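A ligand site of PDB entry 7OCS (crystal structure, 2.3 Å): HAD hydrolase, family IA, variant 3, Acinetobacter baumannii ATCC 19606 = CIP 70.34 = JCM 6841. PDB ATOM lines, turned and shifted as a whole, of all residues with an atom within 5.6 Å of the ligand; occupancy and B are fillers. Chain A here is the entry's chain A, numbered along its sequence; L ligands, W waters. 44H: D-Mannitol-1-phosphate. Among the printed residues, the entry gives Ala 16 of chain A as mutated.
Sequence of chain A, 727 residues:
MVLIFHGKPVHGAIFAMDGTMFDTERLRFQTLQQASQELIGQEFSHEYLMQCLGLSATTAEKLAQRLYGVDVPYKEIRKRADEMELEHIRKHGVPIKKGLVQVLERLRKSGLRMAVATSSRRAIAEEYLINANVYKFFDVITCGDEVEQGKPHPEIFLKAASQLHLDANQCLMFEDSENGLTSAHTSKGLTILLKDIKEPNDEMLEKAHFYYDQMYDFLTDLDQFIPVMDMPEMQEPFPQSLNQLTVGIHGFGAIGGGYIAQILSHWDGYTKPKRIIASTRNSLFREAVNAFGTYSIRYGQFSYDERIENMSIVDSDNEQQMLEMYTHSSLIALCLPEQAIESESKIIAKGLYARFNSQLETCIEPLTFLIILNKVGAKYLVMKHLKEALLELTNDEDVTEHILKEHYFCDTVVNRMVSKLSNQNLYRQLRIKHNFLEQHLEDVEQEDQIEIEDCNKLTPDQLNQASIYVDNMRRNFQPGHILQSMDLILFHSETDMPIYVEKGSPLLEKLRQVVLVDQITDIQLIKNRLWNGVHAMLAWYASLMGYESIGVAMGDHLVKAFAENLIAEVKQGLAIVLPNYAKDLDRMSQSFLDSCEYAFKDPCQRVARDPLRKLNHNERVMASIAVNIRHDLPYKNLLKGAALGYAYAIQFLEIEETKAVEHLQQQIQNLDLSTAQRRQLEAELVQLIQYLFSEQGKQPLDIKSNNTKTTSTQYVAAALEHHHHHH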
ATOM      1  N   ALA A  16     -34.166  11.648   3.404  1.00  0.00           N
ATOM      2  CA  ALA A  16     -33.612  10.613   2.533  1.00  0.00           C
ATOM      3  C   ALA A  16     -34.532   9.386   2.765  1.00  0.00           C
ATOM      4  O   ALA A  16     -35.085   9.232   3.868  1.00  0.00           O
ATOM      5  CB  ALA A  16     -32.194  10.275   2.937  1.00  0.00           C
ATOM      6  N   MET A  17     -34.730   8.553   1.753  1.00  0.00           N
ATOM      7  CA  MET A  17     -35.633   7.413   1.882  1.00  0.00           C
ATOM      8  C   MET A  17     -34.947   6.139   2.426  1.00  0.00           C
ATOM      9  O   MET A  17     -35.262   5.709   3.525  1.00  0.00           O
ATOM     10  CB  MET A  17     -36.371   7.163   0.569  1.00  0.00           C
ATOM     11  CG  MET A  17     -37.331   6.036   0.655  1.00  0.00           C
ATOM     12  SD  MET A  17     -38.056   5.636  -0.941  1.00  0.00           S
ATOM     13  CE  MET A  17     -36.607   5.116  -1.829  1.00  0.00           C
ATOM     14  N   ASP A  18     -34.000   5.564   1.678  1.00  0.00           N
ATOM     15  CA  ASP A  18     -33.348   4.332   2.087  1.00  0.00           C
ATOM     16  C   ASP A  18     -32.340   4.546   3.222  1.00  0.00           C
ATOM     17  O   ASP A  18     -31.419   5.351   3.093  1.00  0.00           O
ATOM     18  CB  ASP A  18     -32.698   3.633   0.888  1.00  0.00           C
ATOM     19  CG  ASP A  18     -33.724   3.239  -0.168  1.00  0.00           C
ATOM     20  OD1 ASP A  18     -34.792   2.728   0.219  1.00  0.00           O
ATOM     21  OD2 ASP A  18     -33.446   3.430  -1.357  1.00  0.00           O
ATOM     22  N   GLY A  19     -32.556   3.841   4.313  1.00  0.00           N
ATOM     23  CA  GLY A  19     -31.697   3.931   5.494  1.00  0.00           C
ATOM     24  C   GLY A  19     -32.140   4.973   6.500  1.00  0.00           C
ATOM     25  O   GLY A  19     -31.697   4.949   7.656  1.00  0.00           O
ATOM     26  N   THR A  20     -33.005   5.908   6.088  1.00  0.00           N
ATOM     27  CA  THR A  20     -33.478   6.969   6.954  1.00  0.00           C
ATOM     28  C   THR A  20     -34.960   6.720   7.310  1.00  0.00           C
ATOM     29  O   THR A  20     -35.314   6.594   8.486  1.00  0.00           O
ATOM     30  CB  THR A  20     -33.235   8.349   6.285  1.00  0.00           C
ATOM     31  OG1 THR A  20     -31.881   8.440   5.893  1.00  0.00           O
ATOM     32  CG2 THR A  20     -33.601   9.484   7.167  1.00  0.00           C
ATOM     33  N   GLU A  25     -31.606  -0.659   3.439  1.00  0.00           N
ATOM     34  CA  GLU A  25     -30.184  -0.806   3.076  1.00  0.00           C
ATOM     35  C   GLU A  25     -29.653  -2.159   3.469  1.00  0.00           C
ATOM     36  O   GLU A  25     -28.830  -2.707   2.754  1.00  0.00           O
ATOM     37  CB  GLU A  25     -29.321   0.325   3.670  1.00  0.00           C
ATOM     38  CG  GLU A  25     -29.688   1.705   3.174  1.00  0.00           C
ATOM     39  CD  GLU A  25     -29.175   2.056   1.799  1.00  0.00           C
ATOM     40  OE1 GLU A  25     -28.846   1.139   1.014  1.00  0.00           O
ATOM     41  OE2 GLU A  25     -29.084   3.267   1.491  1.00  0.00           O
ATOM     42  N   ARG A  28     -30.939  -4.583   0.890  1.00  0.00           N
ATOM     43  CA  ARG A  28     -30.215  -4.339  -0.354  1.00  0.00           C
ATOM     44  C   ARG A  28     -28.794  -4.889  -0.308  1.00  0.00           C
ATOM     45  O   ARG A  28     -28.279  -5.333  -1.332  1.00  0.00           O
ATOM     46  CB  ARG A  28     -30.204  -2.859  -0.679  1.00  0.00           C
ATOM     47  CG  ARG A  28     -30.049  -2.591  -2.159  1.00  0.00           C
ATOM     48  CD  ARG A  28     -30.453  -1.195  -2.489  1.00  0.00           C
ATOM     49  NE  ARG A  28     -31.888  -0.966  -2.283  1.00  0.00           N
ATOM     50  CZ  ARG A  28     -32.445   0.244  -2.250  1.00  0.00           C
ATOM     51  NH1 ARG A  28     -31.701   1.344  -2.376  1.00  0.00           N
ATOM     52  NH2 ARG A  28     -33.754   0.365  -2.093  1.00  0.00           N
ATOM     53  N   LEU A  32     -27.820  -7.522  -3.306  1.00  0.00           N
ATOM     54  CA  LEU A  32     -26.634  -7.201  -4.124  1.00  0.00           C
ATOM     55  C   LEU A  32     -25.529  -8.240  -3.948  1.00  0.00           C
ATOM     56  O   LEU A  32     -24.816  -8.523  -4.898  1.00  0.00           O
ATOM     57  CB  LEU A  32     -26.107  -5.803  -3.794  1.00  0.00           C
ATOM     58  CG  LEU A  32     -26.929  -4.661  -4.355  1.00  0.00           C
ATOM     59  CD1 LEU A  32     -26.530  -3.359  -3.729  1.00  0.00           C
ATOM     60  CD2 LEU A  32     -26.781  -4.580  -5.854  1.00  0.00           C
ATOM     61  N   LEU A  49     -20.053  -2.190  -0.626  1.00  0.00           N
ATOM     62  CA  LEU A  49     -21.438  -1.892  -0.282  1.00  0.00           C
ATOM     63  C   LEU A  49     -21.582  -0.730   0.726  1.00  0.00           C
ATOM     64  O   LEU A  49     -22.558   0.019   0.647  1.00  0.00           O
ATOM     65  CB  LEU A  49     -22.156  -3.144   0.192  1.00  0.00           C
ATOM     66  CG  LEU A  49     -22.243  -4.281  -0.854  1.00  0.00           C
ATOM     67  CD1 LEU A  49     -22.796  -5.548  -0.245  1.00  0.00           C
ATOM     68  CD2 LEU A  49     -23.086  -3.850  -2.041  1.00  0.00           C
ATOM     69  N   CYS A  52     -21.088   2.535  -1.145  1.00  0.00           N
ATOM     70  CA  CYS A  52     -22.267   2.791  -1.986  1.00  0.00           C
ATOM     71  C   CYS A  52     -23.389   3.500  -1.304  1.00  0.00           C
ATOM     72  O   CYS A  52     -24.310   3.977  -1.982  1.00  0.00           O
ATOM     73  CB  CYS A  52     -22.757   1.491  -2.610  1.00  0.00           C
ATOM     74  SG  CYS A  52     -21.770   0.932  -3.988  1.00  0.00           S
ATOM     75  N   LEU A  53     -23.399   3.518   0.036  1.00  0.00           N
ATOM     76  CA  LEU A  53     -24.465   4.147   0.794  1.00  0.00           C
ATOM     77  C   LEU A  53     -24.642   5.629   0.424  1.00  0.00           C
ATOM     78  O   LEU A  53     -23.679   6.397   0.430  1.00  0.00           O
ATOM     79  CB  LEU A  53     -24.243   3.962   2.296  1.00  0.00           C
ATOM     80  CG  LEU A  53     -24.270   2.503   2.768  1.00  0.00           C
ATOM     81  CD1 LEU A  53     -23.972   2.388   4.232  1.00  0.00           C
ATOM     82  CD2 LEU A  53     -25.601   1.835   2.439  1.00  0.00           C
ATOM     83  N   GLY A  54     -25.852   5.978   0.002  1.00  0.00           N
ATOM     84  CA  GLY A  54     -26.173   7.325  -0.422  1.00  0.00           C
ATOM     85  C   GLY A  54     -26.000   7.569  -1.913  1.00  0.00           C
ATOM     86  O   GLY A  54     -26.469   8.576  -2.421  1.00  0.00           O
ATOM     87  N   LEU A  55     -25.310   6.653  -2.623  1.00  0.00           N
ATOM     88  CA  LEU A  55     -25.047   6.841  -4.050  1.00  0.00           C
ATOM     89  C   LEU A  55     -26.182   6.355  -4.929  1.00  0.00           C
ATOM     90  O   LEU A  55     -26.862   5.380  -4.595  1.00  0.00           O
ATOM     91  CB  LEU A  55     -23.750   6.141  -4.483  1.00  0.00           C
ATOM     92  CG  LEU A  55     -22.487   6.525  -3.739  1.00  0.00           C
ATOM     93  CD1 LEU A  55     -21.314   5.734  -4.268  1.00  0.00           C
ATOM     94  CD2 LEU A  55     -22.206   8.010  -3.845  1.00  0.00           C
ATOM     95  N   SER A  56     -26.354   6.996  -6.086  1.00  0.00           N
ATOM     96  CA  SER A  56     -27.347   6.549  -7.063  1.00  0.00           C
ATOM     97  C   SER A  56     -26.817   5.318  -7.812  1.00  0.00           C
ATOM     98  O   SER A  56     -25.617   5.017  -7.723  1.00  0.00           O
ATOM     99  CB  SER A  56     -27.649   7.683  -8.044  1.00  0.00           C
ATOM    100  OG  SER A  56     -26.540   7.929  -8.903  1.00  0.00           O
ATOM    101  N   ALA A  60     -22.853   4.313  -8.099  1.00  0.00           N
ATOM    102  CA  ALA A  60     -22.482   3.005  -7.557  1.00  0.00           C
ATOM    103  C   ALA A  60     -21.916   2.094  -8.669  1.00  0.00           C
ATOM    104  O   ALA A  60     -21.052   1.273  -8.386  1.00  0.00           O
ATOM    105  CB  ALA A  60     -23.671   2.357  -6.878  1.00  0.00           C
ATOM    106  N   TYR A  74     -22.472  -4.491 -13.548  1.00  0.00           N
ATOM    107  CA  TYR A  74     -23.217  -3.905 -12.447  1.00  0.00           C
ATOM    108  C   TYR A  74     -24.659  -3.721 -12.803  1.00  0.00           C
ATOM    109  O   TYR A  74     -25.506  -4.007 -11.980  1.00  0.00           O
ATOM    110  CB  TYR A  74     -22.619  -2.582 -11.969  1.00  0.00           C
ATOM    111  CG  TYR A  74     -23.336  -2.029 -10.748  1.00  0.00           C
ATOM    112  CD1 TYR A  74     -23.138  -2.582  -9.493  1.00  0.00           C
ATOM    113  CD2 TYR A  74     -24.297  -1.033 -10.875  1.00  0.00           C
ATOM    114  CE1 TYR A  74     -23.852  -2.134  -8.395  1.00  0.00           C
ATOM    115  CE2 TYR A  74     -24.976  -0.549  -9.768  1.00  0.00           C
ATOM    116  CZ  TYR A  74     -24.752  -1.102  -8.523  1.00  0.00           C
ATOM    117  OH  TYR A  74     -25.430  -0.636  -7.429  1.00  0.00           O
ATOM    118  N   ARG A  78     -27.385  -5.313 -10.421  1.00  0.00           N
ATOM    119  CA  ARG A  78     -28.340  -4.405  -9.793  1.00  0.00           C
ATOM    120  C   ARG A  78     -29.754  -4.727 -10.203  1.00  0.00           C
ATOM    121  O   ARG A  78     -30.639  -4.718  -9.372  1.00  0.00           O
ATOM    122  CB  ARG A  78     -28.010  -2.944 -10.127  1.00  0.00           C
ATOM    123  CG  ARG A  78     -28.861  -1.941  -9.342  1.00  0.00           C
ATOM    124  CD  ARG A  78     -28.597  -2.032  -7.847  1.00  0.00           C
ATOM    125  NE  ARG A  78     -29.510  -1.194  -7.067  1.00  0.00           N
ATOM    126  CZ  ARG A  78     -29.261   0.073  -6.744  1.00  0.00           C
ATOM    127  NH1 ARG A  78     -30.145   0.764  -6.023  1.00  0.00           N
ATOM    128  NH2 ARG A  78     -28.143   0.666  -7.137  1.00  0.00           N
ATOM    129  N   ALA A 117     -35.779  13.274  -0.724  1.00  0.00           N
ATOM    130  CA  ALA A 117     -34.637  13.449  -1.633  1.00  0.00           C
ATOM    131  C   ALA A 117     -33.836  12.160  -1.580  1.00  0.00           C
ATOM    132  O   ALA A 117     -33.022  11.977  -0.675  1.00  0.00           O
ATOM    133  CB  ALA A 117     -33.769  14.623  -1.190  1.00  0.00           C
ATOM    134  N   THR A 118     -34.108  11.236  -2.533  1.00  0.00           N
ATOM    135  CA  THR A 118     -33.485   9.920  -2.537  1.00  0.00           C
ATOM    136  C   THR A 118     -32.624   9.655  -3.755  1.00  0.00           C
ATOM    137  O   THR A 118     -33.027   9.967  -4.866  1.00  0.00           O
ATOM    138  CB  THR A 118     -34.566   8.828  -2.375  1.00  0.00           C
ATOM    139  OG1 THR A 118     -33.947   7.535  -2.388  1.00  0.00           O
ATOM    140  CG2 THR A 118     -35.668   8.910  -3.453  1.00  0.00           C
ATOM    141  N   SER A 119     -31.486   8.982  -3.567  1.00  0.00           N
ATOM    142  CA  SER A 119     -30.645   8.567  -4.673  1.00  0.00           C
ATOM    143  C   SER A 119     -31.306   7.412  -5.497  1.00  0.00           C
ATOM    144  O   SER A 119     -30.849   7.117  -6.601  1.00  0.00           O
ATOM    145  CB  SER A 119     -29.288   8.117  -4.177  1.00  0.00           C
ATOM    146  OG  SER A 119     -28.586   9.200  -3.622  1.00  0.00           O
ATOM    147  N   SER A 120     -32.376   6.755  -4.952  1.00  0.00           N
ATOM    148  CA  SER A 120     -33.101   5.703  -5.654  1.00  0.00           C
ATOM    149  C   SER A 120     -33.888   6.271  -6.813  1.00  0.00           C
ATOM    150  O   SER A 120     -34.259   7.453  -6.777  1.00  0.00           O
ATOM    151  CB  SER A 120     -34.048   4.976  -4.711  1.00  0.00           C
ATOM    152  OG  SER A 120     -33.317   4.164  -3.817  1.00  0.00           O
ATOM    153  N   LYS A 151     -25.678  12.636  -4.900  1.00  0.00           N
ATOM    154  CA  LYS A 151     -24.980  12.676  -3.594  1.00  0.00           C
ATOM    155  C   LYS A 151     -23.547  12.097  -3.738  1.00  0.00           C
ATOM    156  O   LYS A 151     -23.358  11.181  -4.526  1.00  0.00           O
ATOM    157  CB  LYS A 151     -25.796  11.897  -2.525  1.00  0.00           C
ATOM    158  CG  LYS A 151     -27.281  12.307  -2.471  1.00  0.00           C
ATOM    159  CD  LYS A 151     -28.053  11.596  -1.350  1.00  0.00           C
ATOM    160  CE  LYS A 151     -29.542  11.907  -1.397  1.00  0.00           C
ATOM    161  NZ  LYS A 151     -30.300  11.278  -0.279  1.00  0.00           N
ATOM    162  N   GLU A 175     -30.702  12.459   7.255  1.00  0.00           N
ATOM    163  CA  GLU A 175     -29.806  11.555   6.541  1.00  0.00           C
ATOM    164  C   GLU A 175     -29.215  10.466   7.427  1.00  0.00           C
ATOM    165  O   GLU A 175     -29.156  10.605   8.639  1.00  0.00           O
ATOM    166  CB  GLU A 175     -28.704  12.336   5.822  1.00  0.00           C
ATOM    167  CG  GLU A 175     -29.104  12.757   4.413  1.00  0.00           C
ATOM    168  CD  GLU A 175     -29.099  11.647   3.384  1.00  0.00           C
ATOM    169  OE1 GLU A 175     -29.357  11.942   2.200  1.00  0.00           O
ATOM    170  OE2 GLU A 175     -28.831  10.474   3.741  1.00  0.00           O
ATOM    171  N   ASP A 176     -28.742   9.379   6.798  1.00  0.00           N
ATOM    172  CA  ASP A 176     -28.153   8.231   7.480  1.00  0.00           C
ATOM    173  C   ASP A 176     -26.724   7.929   6.948  1.00  0.00           C
ATOM    174  O   ASP A 176     -25.870   7.465   7.689  1.00  0.00           O
ATOM    175  CB  ASP A 176     -29.035   7.005   7.239  1.00  0.00           C
ATOM    176  CG  ASP A 176     -29.145   6.633   5.754  1.00  0.00           C
ATOM    177  OD1 ASP A 176     -29.585   7.501   4.950  1.00  0.00           O
ATOM    178  OD2 ASP A 176     -28.754   5.508   5.403  1.00  0.00           O
ATOM    179  N   SER A 177     -26.497   8.165   5.657  1.00  0.00           N
ATOM    180  CA  SER A 177     -25.220   7.857   5.022  1.00  0.00           C
ATOM    181  C   SER A 177     -24.278   9.030   5.038  1.00  0.00           C
ATOM    182  O   SER A 177     -24.713  10.181   5.068  1.00  0.00           O
ATOM    183  CB  SER A 177     -25.444   7.380   3.593  1.00  0.00           C
ATOM    184  OG  SER A 177     -25.908   8.444   2.789  1.00  0.00           O
HETATM  185  O3P 44H L   1     -32.731   7.567  -0.074  1.00  0.00           O
HETATM  186  P   44H L   1     -31.282   7.339  -0.158  1.00  0.00           P
HETATM  187  O1P 44H L   1     -30.673   7.115   1.316  1.00  0.00           O
HETATM  188  O2P 44H L   1     -30.579   8.600  -0.848  1.00  0.00           O
HETATM  189  O1  44H L   1     -31.022   6.028  -1.022  1.00  0.00           O
HETATM  190  C1  44H L   1     -29.702   5.690  -1.429  1.00  0.00           C
HETATM  191  C2  44H L   1     -29.681   4.233  -1.879  1.00  0.00           C
HETATM  192  O2  44H L   1     -30.329   4.127  -3.161  1.00  0.00           O
HETATM  193  C3  44H L   1     -28.247   3.728  -1.949  1.00  0.00           C
HETATM  194  O3  44H L   1     -27.673   3.764  -0.644  1.00  0.00           O
HETATM  195  C4  44H L   1     -28.193   2.286  -2.467  1.00  0.00           C
HETATM  196  O4  44H L   1     -28.942   1.441  -1.585  1.00  0.00           O
HETATM  197  C5  44H L   1     -26.756   1.763  -2.563  1.00  0.00           C
HETATM  198  C6  44H L   1     -26.727   0.382  -3.195  1.00  0.00           C
HETATM  199  O6  44H L   1     -25.516  -0.276  -2.813  1.00  0.00           O
HETATM  200  O5  44H L   1     -25.968   2.649  -3.371  1.00  0.00           O
HETATM  201  O   HOH W   1     -26.790   2.764  -5.858  1.00  0.00           O
HETATM  202  O   HOH W   2     -29.634   3.792  -5.717  1.00  0.00           O
HETATM  203  O   HOH W   3     -28.327   5.329   2.797  1.00  0.00           O
HETATM  204  O   HOH W   4     -24.871  -0.880  -0.357  1.00  0.00           O
HETATM  205  O   HOH W   5     -28.476   8.574   2.002  1.00  0.00           O
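Ala 16 touches the ligand.
Leu 32 touches the ligand (CD1 to O6, 3.4 Å).
Leu 53 touches the ligand (CA to O3, 3.5 Å).
Asp 176 touches the ligand (OD1 to O1P, 3.8 Å).
Hydrophobic or aromatic side chains within 4 Å of the ligand: Ala 16, Met 17 and Leu 32.
Of the 25 residues printed, 15 come within 4 Å of the ligand.
The nearest printed residue that does not touch the ligand is Ala 117 (4.2 Å).
The side-chain hydroxyl (OG1) of Thr 118 is in hydrogen-bond range of the backbone NH (N) of Ser 120.
OD1 of Asp 176 lies within hydrogen-bond range of OG1 of Thr 20.
OG of Ser 119 sits at hydrogen-bond distance from O of Gly 54.
The backbone carbonyl oxygen of Ala 117 is in hydrogen-bond range of the side-chain amino group of Lys 151 (2.8 Å).
The side-chain carboxylate (OE1) of Glu 175 lies within salt-bridge range of the side-chain amino group (NZ) of Lys 151.
The side-chain carboxylate of Asp 18 is in salt-bridge range of the guanidinium group of Arg 28 (2.9 Å).
The side-chain carboxylate of Asp 18 lies within hydrogen-bond range of the side-chain hydroxyl of Ser 120 (2.6 Å).
Water W4 lies within hydrogen-bond range of an oxygen (O6) of the ligand and the backbone carbonyl oxygen of Leu 49.
Water W1 lies within hydrogen-bond range of O5 of the ligand (2.6 Å), NH2 of Arg 78 (2.8 Å), O of Leu 55 (2.9 Å) and O of Ser 56 (3.2 Å).
Water W2 lies within hydrogen-bond range of an oxygen (O2) of the ligand, the guanidinium group (NH1) of Arg 78 and the backbone carbonyl oxygen (O) of Leu 55.
Water W5 lies within hydrogen-bond range of the side-chain carboxylate of Glu 175 (2.6 Å), the side-chain hydroxyl of Ser 177 (2.7 Å), an oxygen (O1P) of the ligand (2.7 Å) and the side-chain carboxylate of Asp 176 (3.3 Å).
N of Asp 18 lies within hydrogen-bond range of O3P of the ligand, 2.9 Å away.
N of Ser 119 sits at hydrogen-bond distance from O2P of the ligand (2.9 Å).
The side-chain hydroxyl of Ser 120 lies within hydrogen-bond range of an oxygen (O2) of the ligand, 3.1 Å away.
N of Met 17 lies within hydrogen-bond range of O3P of the ligand.
An oxygen (O3) of the ligand sits at hydrogen-bond distance from the backbone NH (N) of Gly 54, 2.9 Å away.
O of Cys 52 is in hydrogen-bond range of O5 of the ligand.
OG1 of Thr 118 is in hydrogen-bond range of O3P of the ligand (2.6 Å).
O of Asp 18 sits close to O1P of the ligand (2.6 Å).
The side-chain carboxylate (OE2) of Glu 25 is in hydrogen-bond range of an oxygen (O3) of the ligand (2.6 Å).
An oxygen (O5) of the ligand sits at hydrogen-bond distance from the backbone carbonyl oxygen (O) of Leu 55 (3.1 Å).
O4 of the ligand is in hydrogen-bond range of NH1 of Arg 28, at 2.9 Å.
The side-chain amino group (NZ) of Lys 151 lies within salt-bridge range of an oxygen (O2P) of the ligand.
An oxygen (O2P) of the ligand sits at hydrogen-bond distance from the side-chain hydroxyl (OG) of Ser 119 (3.5 Å).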
